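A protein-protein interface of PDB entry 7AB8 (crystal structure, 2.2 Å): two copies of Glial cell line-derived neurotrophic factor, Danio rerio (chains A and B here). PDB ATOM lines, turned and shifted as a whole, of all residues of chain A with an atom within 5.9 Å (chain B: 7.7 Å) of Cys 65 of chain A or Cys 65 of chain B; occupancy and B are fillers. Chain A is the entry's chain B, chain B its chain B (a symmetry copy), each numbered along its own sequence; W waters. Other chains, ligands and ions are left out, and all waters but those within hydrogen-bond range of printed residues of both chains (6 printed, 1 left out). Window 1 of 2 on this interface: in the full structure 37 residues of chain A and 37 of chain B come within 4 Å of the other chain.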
ATOM      1  N   CYS A   5       0.335 -14.120  -6.933  1.00  0.00           N
ATOM      2  CA  CYS A   5      -0.756 -14.734  -7.655  1.00  0.00           C
ATOM      3  C   CYS A   5      -1.001 -16.096  -6.993  1.00  0.00           C
ATOM      4  O   CYS A   5      -0.257 -17.008  -7.177  1.00  0.00           O
ATOM      5  CB  CYS A   5      -0.414 -14.880  -9.114  1.00  0.00           C
ATOM      6  SG  CYS A   5      -1.627 -15.786 -10.058  1.00  0.00           S
ATOM      7  N   CYS A  36       0.875  -9.391  -9.761  1.00  0.00           N
ATOM      8  CA  CYS A  36       1.987  -9.929 -10.486  1.00  0.00           C
ATOM      9  C   CYS A  36       3.010  -8.844 -10.862  1.00  0.00           C
ATOM     10  O   CYS A  36       3.761  -9.005 -11.801  1.00  0.00           O
ATOM     11  CB  CYS A  36       1.472 -10.541 -11.768  1.00  0.00           C
ATOM     12  SG  CYS A  36       0.821 -12.168 -11.570  1.00  0.00           S
ATOM     13  N   SER A  62      -2.881  -5.700 -22.302  1.00  0.00           N
ATOM     14  CA  SER A  62      -2.880  -6.303 -20.979  1.00  0.00           C
ATOM     15  C   SER A  62      -1.458  -6.444 -20.455  1.00  0.00           C
ATOM     16  O   SER A  62      -0.558  -6.888 -21.176  1.00  0.00           O
ATOM     17  CB  SER A  62      -3.563  -7.670 -21.022  1.00  0.00           C
ATOM     18  OG  SER A  62      -3.743  -8.190 -19.717  1.00  0.00           O
ATOM     19  N   ARG A  63      -1.257  -6.060 -19.198  1.00  0.00           N
ATOM     20  CA  ARG A  63      -0.005  -6.325 -18.507  1.00  0.00           C
ATOM     21  C   ARG A  63      -0.050  -7.748 -17.951  1.00  0.00           C
ATOM     22  O   ARG A  63      -0.985  -8.509 -18.214  1.00  0.00           O
ATOM     23  CB  ARG A  63       0.239  -5.276 -17.426  1.00  0.00           C
ATOM     24  CG  ARG A  63       0.321  -3.852 -17.958  1.00  0.00           C
ATOM     25  CD  ARG A  63       0.140  -2.832 -16.847  1.00  0.00           C
ATOM     26  NE  ARG A  63       1.275  -2.817 -15.929  1.00  0.00           N
ATOM     27  CZ  ARG A  63       1.265  -2.222 -14.740  1.00  0.00           C
ATOM     28  NH1 ARG A  63       2.343  -2.259 -13.970  1.00  0.00           N
ATOM     29  NH2 ARG A  63       0.176  -1.591 -14.321  1.00  0.00           N
ATOM     30  N   THR A  64       0.963  -8.120 -17.172  1.00  0.00           N
ATOM     31  CA  THR A  64       1.052  -9.478 -16.646  1.00  0.00           C
ATOM     32  C   THR A  64      -0.192  -9.830 -15.840  1.00  0.00           C
ATOM     33  O   THR A  64      -0.599  -9.089 -14.942  1.00  0.00           O
ATOM     34  CB  THR A  64       2.304  -9.628 -15.780  1.00  0.00           C
ATOM     35  OG1 THR A  64       3.438  -9.107 -16.484  1.00  0.00           O
ATOM     36  CG2 THR A  64       2.552 -11.092 -15.452  1.00  0.00           C
ATOM     37  N   CYS A  65      -0.799 -10.966 -16.173  1.00  0.00           N
ATOM     38  CA  CYS A  65      -2.042 -11.409 -15.562  1.00  0.00           C
ATOM     39  C   CYS A  65      -1.792 -12.567 -14.603  1.00  0.00           C
ATOM     40  O   CYS A  65      -0.895 -13.389 -14.814  1.00  0.00           O
ATOM     41  CB  CYS A  65      -3.059 -11.847 -16.624  1.00  0.00           C
ATOM     42  SG  CYS A  65      -3.567 -10.566 -17.793  1.00  0.00           S
ATOM     43  N   CYS A  66      -2.597 -12.619 -13.545  1.00  0.00           N
ATOM     44  CA  CYS A  66      -2.632 -13.759 -12.637  1.00  0.00           C
ATOM     45  C   CYS A  66      -3.676 -14.737 -13.164  1.00  0.00           C
ATOM     46  O   CYS A  66      -4.881 -14.500 -13.034  1.00  0.00           O
ATOM     47  CB  CYS A  66      -2.961 -13.307 -11.217  1.00  0.00           C
ATOM     48  SG  CYS A  66      -3.336 -14.655 -10.077  1.00  0.00           S
ATOM     49  N   ARG A  67      -3.217 -15.830 -13.754  1.00  0.00           N
ATOM     50  CA  ARG A  67      -4.073 -16.704 -14.537  1.00  0.00           C
ATOM     51  C   ARG A  67      -3.804 -18.157 -14.186  1.00  0.00           C
ATOM     52  O   ARG A  67      -2.724 -18.495 -13.690  1.00  0.00           O
ATOM     53  CB  ARG A  67      -3.845 -16.486 -16.039  1.00  0.00           C
ATOM     54  CG  ARG A  67      -4.424 -15.192 -16.571  1.00  0.00           C
ATOM     55  CD  ARG A  67      -5.890 -15.359 -16.890  1.00  0.00           C
ATOM     56  NE  ARG A  67      -6.107 -16.460 -17.823  1.00  0.00           N
ATOM     57  CZ  ARG A  67      -7.267 -17.086 -17.981  1.00  0.00           C
ATOM     58  NH1 ARG A  67      -8.321 -16.719 -17.267  1.00  0.00           N
ATOM     59  NH2 ARG A  67      -7.372 -18.079 -18.853  1.00  0.00           N
ATOM     60  N   ALA A  96      -0.123 -18.847 -12.003  1.00  0.00           N
ATOM     61  CA  ALA A  96       1.132 -18.244 -12.464  1.00  0.00           C
ATOM     62  C   ALA A  96       0.899 -16.882 -13.065  1.00  0.00           C
ATOM     63  O   ALA A  96      -0.168 -16.583 -13.513  1.00  0.00           O
ATOM     64  CB  ALA A  96       1.858 -19.071 -13.490  1.00  0.00           C
ATOM     65  N   CYS A  97       1.945 -16.073 -13.076  1.00  0.00           N
ATOM     66  CA  CYS A  97       1.894 -14.779 -13.661  1.00  0.00           C
ATOM     67  C   CYS A  97       2.212 -14.991 -15.158  1.00  0.00           C
ATOM     68  O   CYS A  97       3.217 -15.536 -15.495  1.00  0.00           O
ATOM     69  CB  CYS A  97       2.892 -13.869 -12.978  1.00  0.00           C
ATOM     70  SG  CYS A  97       2.406 -13.398 -11.322  1.00  0.00           S
ATOM     71  N   VAL A  98       1.325 -14.570 -16.037  1.00  0.00           N
ATOM     72  CA  VAL A  98       1.455 -14.789 -17.473  1.00  0.00           C
ATOM     73  C   VAL A  98       1.318 -13.480 -18.241  1.00  0.00           C
ATOM     74  O   VAL A  98       1.778 -13.369 -19.377  1.00  0.00           O
ATOM     75  CB  VAL A  98       0.419 -15.809 -17.968  1.00  0.00           C
ATOM     76  CG1 VAL A  98       0.599 -17.143 -17.257  1.00  0.00           C
ATOM     77  CG2 VAL A  98      -0.983 -15.272 -17.749  1.00  0.00           C
ATOM     78  OXT VAL A  98       0.740 -12.507 -17.755  1.00  0.00           O
ATOM     79  N   CYS B   5      -6.192 -11.907 -30.802  1.00  0.00           N
ATOM     80  CA  CYS B   5      -5.052 -11.362 -30.100  1.00  0.00           C
ATOM     81  C   CYS B   5      -3.913 -11.276 -31.125  1.00  0.00           C
ATOM     82  O   CYS B   5      -3.333 -12.254 -31.478  1.00  0.00           O
ATOM     83  CB  CYS B   5      -4.680 -12.235 -28.930  1.00  0.00           C
ATOM     84  SG  CYS B   5      -3.177 -11.742 -28.104  1.00  0.00           S
ATOM     85  N   CYS B  32       1.002  -6.888 -27.812  1.00  0.00           N
ATOM     86  CA  CYS B  32      -0.098  -7.795 -28.105  1.00  0.00           C
ATOM     87  C   CYS B  32      -1.410  -7.154 -27.678  1.00  0.00           C
ATOM     88  O   CYS B  32      -1.533  -6.676 -26.544  1.00  0.00           O
ATOM     89  CB  CYS B  32       0.093  -9.134 -27.393  1.00  0.00           C
ATOM     90  SG  CYS B  32       1.517 -10.074 -27.974  1.00  0.00           S
ATOM     91  N   GLY B  34      -5.945  -7.327 -28.533  1.00  0.00           N
ATOM     92  CA  GLY B  34      -7.071  -7.963 -29.175  1.00  0.00           C
ATOM     93  C   GLY B  34      -7.898  -8.792 -28.214  1.00  0.00           C
ATOM     94  O   GLY B  34      -7.469  -9.110 -27.100  1.00  0.00           O
ATOM     95  N   PRO B  35      -9.104  -9.161 -28.630  1.00  0.00           N
ATOM     96  CA  PRO B  35      -9.972  -9.967 -27.770  1.00  0.00           C
ATOM     97  C   PRO B  35      -9.590 -11.440 -27.802  1.00  0.00           C
ATOM     98  O   PRO B  35      -9.003 -11.944 -28.761  1.00  0.00           O
ATOM     99  CB  PRO B  35     -11.363  -9.746 -28.375  1.00  0.00           C
ATOM    100  CG  PRO B  35     -11.087  -9.529 -29.827  1.00  0.00           C
ATOM    101  CD  PRO B  35      -9.753  -8.822 -29.911  1.00  0.00           C
ATOM    102  N   CYS B  36      -9.894 -12.124 -26.691  1.00  0.00           N
ATOM    103  CA  CYS B  36      -9.647 -13.524 -26.518  1.00  0.00           C
ATOM    104  C   CYS B  36     -10.903 -14.277 -26.046  1.00  0.00           C
ATOM    105  O   CYS B  36     -10.803 -15.330 -25.453  1.00  0.00           O
ATOM    106  CB  CYS B  36      -8.583 -13.696 -25.458  1.00  0.00           C
ATOM    107  SG  CYS B  36      -6.939 -13.486 -26.058  1.00  0.00           S
ATOM    108  N   ALA B  39     -11.359 -18.054 -26.883  1.00  0.00           N
ATOM    109  CA  ALA B  39     -10.477 -18.994 -26.236  1.00  0.00           C
ATOM    110  C   ALA B  39     -10.812 -19.122 -24.744  1.00  0.00           C
ATOM    111  O   ALA B  39     -10.109 -19.747 -24.033  1.00  0.00           O
ATOM    112  CB  ALA B  39      -9.039 -18.567 -26.406  1.00  0.00           C
ATOM    113  N   GLU B  40     -11.909 -18.552 -24.292  1.00  0.00           N
ATOM    114  CA  GLU B  40     -12.245 -18.633 -22.882  1.00  0.00           C
ATOM    115  C   GLU B  40     -12.849 -19.992 -22.544  1.00  0.00           C
ATOM    116  O   GLU B  40     -13.272 -20.756 -23.417  1.00  0.00           O
ATOM    117  CB  GLU B  40     -13.220 -17.527 -22.486  1.00  0.00           C
ATOM    118  CG  GLU B  40     -12.727 -16.111 -22.713  1.00  0.00           C
ATOM    119  CD  GLU B  40     -13.480 -15.102 -21.864  1.00  0.00           C
ATOM    120  OE1 GLU B  40     -12.846 -14.450 -21.008  1.00  0.00           O
ATOM    121  OE2 GLU B  40     -14.707 -14.966 -22.046  1.00  0.00           O
ATOM    122  N   ASP B  44     -13.567 -18.919 -17.179  1.00  0.00           N
ATOM    123  CA  ASP B  44     -13.690 -17.500 -17.493  1.00  0.00           C
ATOM    124  C   ASP B  44     -15.146 -17.048 -17.464  1.00  0.00           C
ATOM    125  O   ASP B  44     -15.446 -15.936 -17.017  1.00  0.00           O
ATOM    126  CB  ASP B  44     -13.062 -17.209 -18.857  1.00  0.00           C
ATOM    127  CG  ASP B  44     -11.562 -17.435 -18.867  1.00  0.00           C
ATOM    128  OD1 ASP B  44     -10.856 -16.771 -18.081  1.00  0.00           O
ATOM    129  OD2 ASP B  44     -11.089 -18.275 -19.660  1.00  0.00           O
ATOM    130  N   SER B  62      -8.596 -12.307 -13.153  1.00  0.00           N
ATOM    131  CA  SER B  62      -8.394 -11.994 -14.558  1.00  0.00           C
ATOM    132  C   SER B  62      -8.935 -13.110 -15.440  1.00  0.00           C
ATOM    133  O   SER B  62      -8.694 -14.294 -15.182  1.00  0.00           O
ATOM    134  CB  SER B  62      -6.909 -11.772 -14.841  1.00  0.00           C
ATOM    135  OG  SER B  62      -6.709 -11.281 -16.154  1.00  0.00           O
ATOM    136  N   ARG B  63      -9.672 -12.730 -16.479  1.00  0.00           N
ATOM    137  CA  ARG B  63     -10.080 -13.669 -17.513  1.00  0.00           C
ATOM    138  C   ARG B  63      -8.935 -13.815 -18.514  1.00  0.00           C
ATOM    139  O   ARG B  63      -7.839 -13.283 -18.317  1.00  0.00           O
ATOM    140  CB  ARG B  63     -11.381 -13.209 -18.165  1.00  0.00           C
ATOM    141  CG  ARG B  63     -12.547 -13.088 -17.193  1.00  0.00           C
ATOM    142  CD  ARG B  63     -13.670 -12.246 -17.775  1.00  0.00           C
ATOM    143  NE  ARG B  63     -14.342 -12.922 -18.881  1.00  0.00           N
ATOM    144  CZ  ARG B  63     -15.170 -12.321 -19.730  1.00  0.00           C
ATOM    145  NH1 ARG B  63     -15.736 -13.014 -20.708  1.00  0.00           N
ATOM    146  NH2 ARG B  63     -15.430 -11.027 -19.601  1.00  0.00           N
ATOM    147  N   THR B  64      -9.181 -14.538 -19.605  1.00  0.00           N
ATOM    148  CA  THR B  64      -8.137 -14.796 -20.591  1.00  0.00           C
ATOM    149  C   THR B  64      -7.560 -13.492 -21.125  1.00  0.00           C
ATOM    150  O   THR B  64      -8.297 -12.601 -21.560  1.00  0.00           O
ATOM    151  CB  THR B  64      -8.692 -15.640 -21.739  1.00  0.00           C
ATOM    152  OG1 THR B  64      -9.404 -16.764 -21.206  1.00  0.00           O
ATOM    153  CG2 THR B  64      -7.563 -16.141 -22.626  1.00  0.00           C
ATOM    154  N   CYS B  65      -6.235 -13.380 -21.084  1.00  0.00           N
ATOM    155  CA  CYS B  65      -5.529 -12.171 -21.478  1.00  0.00           C
ATOM    156  C   CYS B  65      -4.834 -12.363 -22.820  1.00  0.00           C
ATOM    157  O   CYS B  65      -4.384 -13.463 -23.156  1.00  0.00           O
ATOM    158  CB  CYS B  65      -4.488 -11.768 -20.425  1.00  0.00           C
ATOM    159  SG  CYS B  65      -5.143 -11.389 -18.784  1.00  0.00           S
ATOM    160  N   CYS B  66      -4.754 -11.276 -23.584  1.00  0.00           N
ATOM    161  CA  CYS B  66      -3.954 -11.226 -24.802  1.00  0.00           C
ATOM    162  C   CYS B  66      -2.558 -10.753 -24.419  1.00  0.00           C
ATOM    163  O   CYS B  66      -2.349  -9.567 -24.144  1.00  0.00           O
ATOM    164  CB  CYS B  66      -4.594 -10.297 -25.829  1.00  0.00           C
ATOM    165  SG  CYS B  66      -3.540  -9.917 -27.244  1.00  0.00           S
ATOM    166  N   ARG B  67      -1.605 -11.673 -24.401  1.00  0.00           N
ATOM    167  CA  ARG B  67      -0.306 -11.431 -23.797  1.00  0.00           C
ATOM    168  C   ARG B  67       0.799 -11.940 -24.706  1.00  0.00           C
ATOM    169  O   ARG B  67       0.570 -12.815 -25.547  1.00  0.00           O
ATOM    170  CB  ARG B  67      -0.205 -12.118 -22.429  1.00  0.00           C
ATOM    171  CG  ARG B  67      -1.007 -11.442 -21.337  1.00  0.00           C
ATOM    172  CD  ARG B  67      -0.227 -10.296 -20.739  1.00  0.00           C
ATOM    173  NE  ARG B  67       1.072 -10.740 -20.246  1.00  0.00           N
ATOM    174  CZ  ARG B  67       2.106  -9.933 -20.036  1.00  0.00           C
ATOM    175  NH1 ARG B  67       1.993  -8.635 -20.276  1.00  0.00           N
ATOM    176  NH2 ARG B  67       3.252 -10.425 -19.586  1.00  0.00           N
ATOM    177  N   PRO B  68       2.014 -11.411 -24.558  1.00  0.00           N
ATOM    178  CA  PRO B  68       3.150 -11.975 -25.295  1.00  0.00           C
ATOM    179  C   PRO B  68       3.598 -13.294 -24.689  1.00  0.00           C
ATOM    180  O   PRO B  68       3.641 -13.460 -23.468  1.00  0.00           O
ATOM    181  CB  PRO B  68       4.232 -10.899 -25.151  1.00  0.00           C
ATOM    182  CG  PRO B  68       3.895 -10.205 -23.875  1.00  0.00           C
ATOM    183  CD  PRO B  68       2.390 -10.201 -23.805  1.00  0.00           C
ATOM    184  N   CYS B  95       2.224 -13.465 -29.935  1.00  0.00           N
ATOM    185  CA  CYS B  95       1.083 -13.279 -29.052  1.00  0.00           C
ATOM    186  C   CYS B  95       0.309 -14.578 -28.895  1.00  0.00           C
ATOM    187  O   CYS B  95       0.457 -15.514 -29.684  1.00  0.00           O
ATOM    188  CB  CYS B  95       0.161 -12.186 -29.598  1.00  0.00           C
ATOM    189  SG  CYS B  95       0.982 -10.610 -29.852  1.00  0.00           S
ATOM    190  N   ALA B  96      -0.519 -14.620 -27.848  1.00  0.00           N
ATOM    191  CA  ALA B  96      -1.411 -15.741 -27.534  1.00  0.00           C
ATOM    192  C   ALA B  96      -2.386 -15.381 -26.443  1.00  0.00           C
ATOM    193  O   ALA B  96      -2.139 -14.509 -25.662  1.00  0.00           O
ATOM    194  CB  ALA B  96      -0.686 -16.985 -27.097  1.00  0.00           C
ATOM    195  N   CYS B  97      -3.497 -16.096 -26.406  1.00  0.00           N
ATOM    196  CA  CYS B  97      -4.483 -15.911 -25.400  1.00  0.00           C
ATOM    197  C   CYS B  97      -4.034 -16.793 -24.214  1.00  0.00           C
ATOM    198  O   CYS B  97      -3.839 -17.960 -24.363  1.00  0.00           O
ATOM    199  CB  CYS B  97      -5.842 -16.306 -25.936  1.00  0.00           C
ATOM    200  SG  CYS B  97      -6.499 -15.145 -27.129  1.00  0.00           S
ATOM    201  N   VAL B  98      -3.854 -16.206 -23.048  1.00  0.00           N
ATOM    202  CA  VAL B  98      -3.343 -16.901 -21.872  1.00  0.00           C
ATOM    203  C   VAL B  98      -4.264 -16.700 -20.674  1.00  0.00           C
ATOM    204  O   VAL B  98      -4.247 -17.491 -19.732  1.00  0.00           O
ATOM    205  CB  VAL B  98      -1.919 -16.434 -21.534  1.00  0.00           C
ATOM    206  CG1 VAL B  98      -0.978 -16.700 -22.701  1.00  0.00           C
ATOM    207  CG2 VAL B  98      -1.928 -14.958 -21.181  1.00  0.00           C
ATOM    208  OXT VAL B  98      -5.038 -15.744 -20.612  1.00  0.00           O
HETATM  209  O   HOH W   1       5.670 -10.731 -17.326  1.00  0.00           O
HETATM  210  O   HOH W   2      -3.289  -7.331 -24.635  1.00  0.00           O
HETATM  211  O   HOH W   3      -7.748 -15.829 -13.185  1.00  0.00           O
HETATM  212  O   HOH W   4      -6.398 -13.231 -11.546  1.00  0.00           O
HETATM  213  O   HOH W   5      -8.579 -19.501 -21.605  1.00  0.00           O
HETATM  214  O   HOH W   6       2.411 -15.008 -21.277  1.00  0.00           O
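Of the 11 printed residues of chain A, 7 touch a printed residue of chain B.
Of the 19 printed residues of chain B, 8 touch a printed residue of chain A.
Printed residues of chain B that touch a printed residue of chain A: Asp 44, Ser 62, Arg 63, Thr 64, Cys 65, Cys 66, Arg 67 and Val 98.
Hydrophobic or aromatic side chains of chain B that line the printed part of chain A: Val 98.
Along chain B the printed residues that touch a printed residue of chain A span positions 44 to 98.
Among the printed residues, 15 pairs touch across the chains.
Among the printed residues, Asp or Glu carboxylates within 4 Å of a Lys or Arg side-chain nitrogen of the other chain: Arg 67 of chain A with Asp 44 of chain B (2.7 Å).
Ser 62 of chain A touches Cys 66 of chain B, and with the chains exchanged Cys 66 of chain A touches Ser 62 of chain B.
Ser 62 of chain A touches Arg 67 of chain B, and with the chains exchanged Arg 67 of chain A touches Ser 62 of chain B.
Arg 63 of chain A touches Arg 67 of chain B, and with the chains exchanged Arg 67 of chain A touches Arg 63 of chain B.
Arg 67 of chain A touches Val 98 of chain B, and with the chains exchanged Val 98 of chain A touches Arg 67 of chain B.
Of the 15 pairs that touch across the chains among the printed residues, 14 have their exchanged pair printed and touching as well.
The side-chain sulfur of Cys 65 of chain A sits at hydrogen-bond distance from the side-chain hydroxyl of Ser 62 of chain B (3.6 Å).
NH2 of Arg 67 of chain A sits at hydrogen-bond distance from OG1 of Thr 64 of chain B, at 3.4 Å.
The guanidinium group (NH1) of Arg 67 of chain B lies within hydrogen-bond range of the backbone carbonyl oxygen (O) of Ser 62 of chain A, at 3.2 Å.
OG of Ser 62 of chain A sits at hydrogen-bond distance from SG of Cys 65 of chain B (3.6 Å).
SG of Cys 65 of chain A forms a disulfide with SG of Cys 65 of chain B.
The guanidinium group (NH2) of Arg 67 of chain B sits at hydrogen-bond distance from the side-chain hydroxyl (OG1) of Thr 64 of chain A (3.4 Å).
NH1 of Arg 67 of chain A lies within hydrogen-bond range of O of Ser 62 of chain B (3.2 Å).
The guanidinium group (NH1) of Arg 67 of chain A is in salt-bridge range of the side-chain carboxylate (OD1) of Asp 44 of chain B, at 2.7 Å.
NE of Arg 67 of chain B is in salt-bridge range of O of Val 98 of chain A.
The guanidinium group of Arg 67 of chain A lies within salt-bridge range of the chain-end carboxylate of Val 98 of chain B.
SG of Cys 95 of chain B forms a disulfide with SG of Cys 32 of chain B.
The backbone NH (N) of Ala 96 of chain B lies within hydrogen-bond range of the backbone carbonyl oxygen (O) of Arg 67 of chain B (3.1 Å).
The side-chain carboxylate (OD2) of Asp 44 of chain B lies within hydrogen-bond range of the side-chain hydroxyl (OG1) of Thr 64 of chain B, 2.7 Å away.
The backbone NH (N) of Gly 34 of chain B is in hydrogen-bond range of the side-chain sulfur (SG) of Cys 66 of chain B (3.8 Å).
SG of Cys 97 of chain A is disulfide-bonded to SG of Cys 36 of chain A.
The side-chain sulfur (SG) of Cys 66 of chain B forms a disulfide with the side-chain sulfur (SG) of Cys 5 of chain B, at 2.0 Å.
Water W4 lies within hydrogen-bond range of the backbone carbonyl oxygen (O) of Cys 66 of chain A (2.5 Å) and the backbone NH (N) of Ser 62 of chain B (2.9 Å).
Water W2 lies within hydrogen-bond range of O of Cys 66 of chain B (2.5 Å), O of Cys 32 of chain B (2.7 Å) and N of Ser 62 of chain A (2.9 Å).
Water W6 bridges the chain-end carboxylate (O) of Val 98 of chain A (2.6 Å) and the backbone carbonyl oxygen (O) of Pro 68 of chain B (3.0 Å).
Water W3 lies within hydrogen-bond range of O of Ser 62 of chain B (2.7 Å) and O of Cys 66 of chain A (3.2 Å).
Water W5 lies within hydrogen-bond range of the backbone carbonyl oxygen of Ala 39 of chain B (2.9 Å), the side-chain hydroxyl of Thr 64 of chain B (2.9 Å), the guanidinium group of Arg 67 of chain A (3.3 Å) and the side-chain carboxylate of Asp 44 of chain B (3.4 Å).
Water W1 bridges OG1 of Thr 64 of chain A (2.9 Å) and NH2 of Arg 67 of chain B (3.3 Å).
Cys 5 of chain A touches none of the printed residues of chain B.
Printed residues of chain B within 4 Å of Ser 62 of chain A: Cys 65 (3.6 Å), Cys 66 (3.8 Å) and Arg 67 (3.2 Å).
Cys 65 of chain A touches two residues of chain B.
Of the printed residues of chain A, Arg 63 of chain B touches Arg 67.
Of the printed residues of chain A, Thr 64 of chain B touches Arg 67 (3.3 Å).
Cys 65 of chain B touches just these residues of chain A: Ser 62 (3.6 Å) and Cys 65 (2.0 Å).
Of the printed residues of chain A, Cys 66 of chain B touches Ser 62.
Printed residues of chain A within 4 Å of Val 98 of chain B: Arg 67 (2.9 Å) and Val 98 (3.6 Å).
The nearest residue of chain B that does not touch Cys 65 of chain A is Arg 67 of chain B (4.5 Å).
Among the printed residues, merely in contact across the chains: Arg 63 of chain A with Arg 67 of chain B (3.2 Å), Arg 67 of chain A with Arg 63 of chain B (3.2 Å), Val 98 of chain A with Val 98 of chain B (3.6 Å), Ser 62 of chain A with Cys 66 of chain B (3.8 Å) and Cys 66 of chain A with Ser 62 of chain B (3.8 Å).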
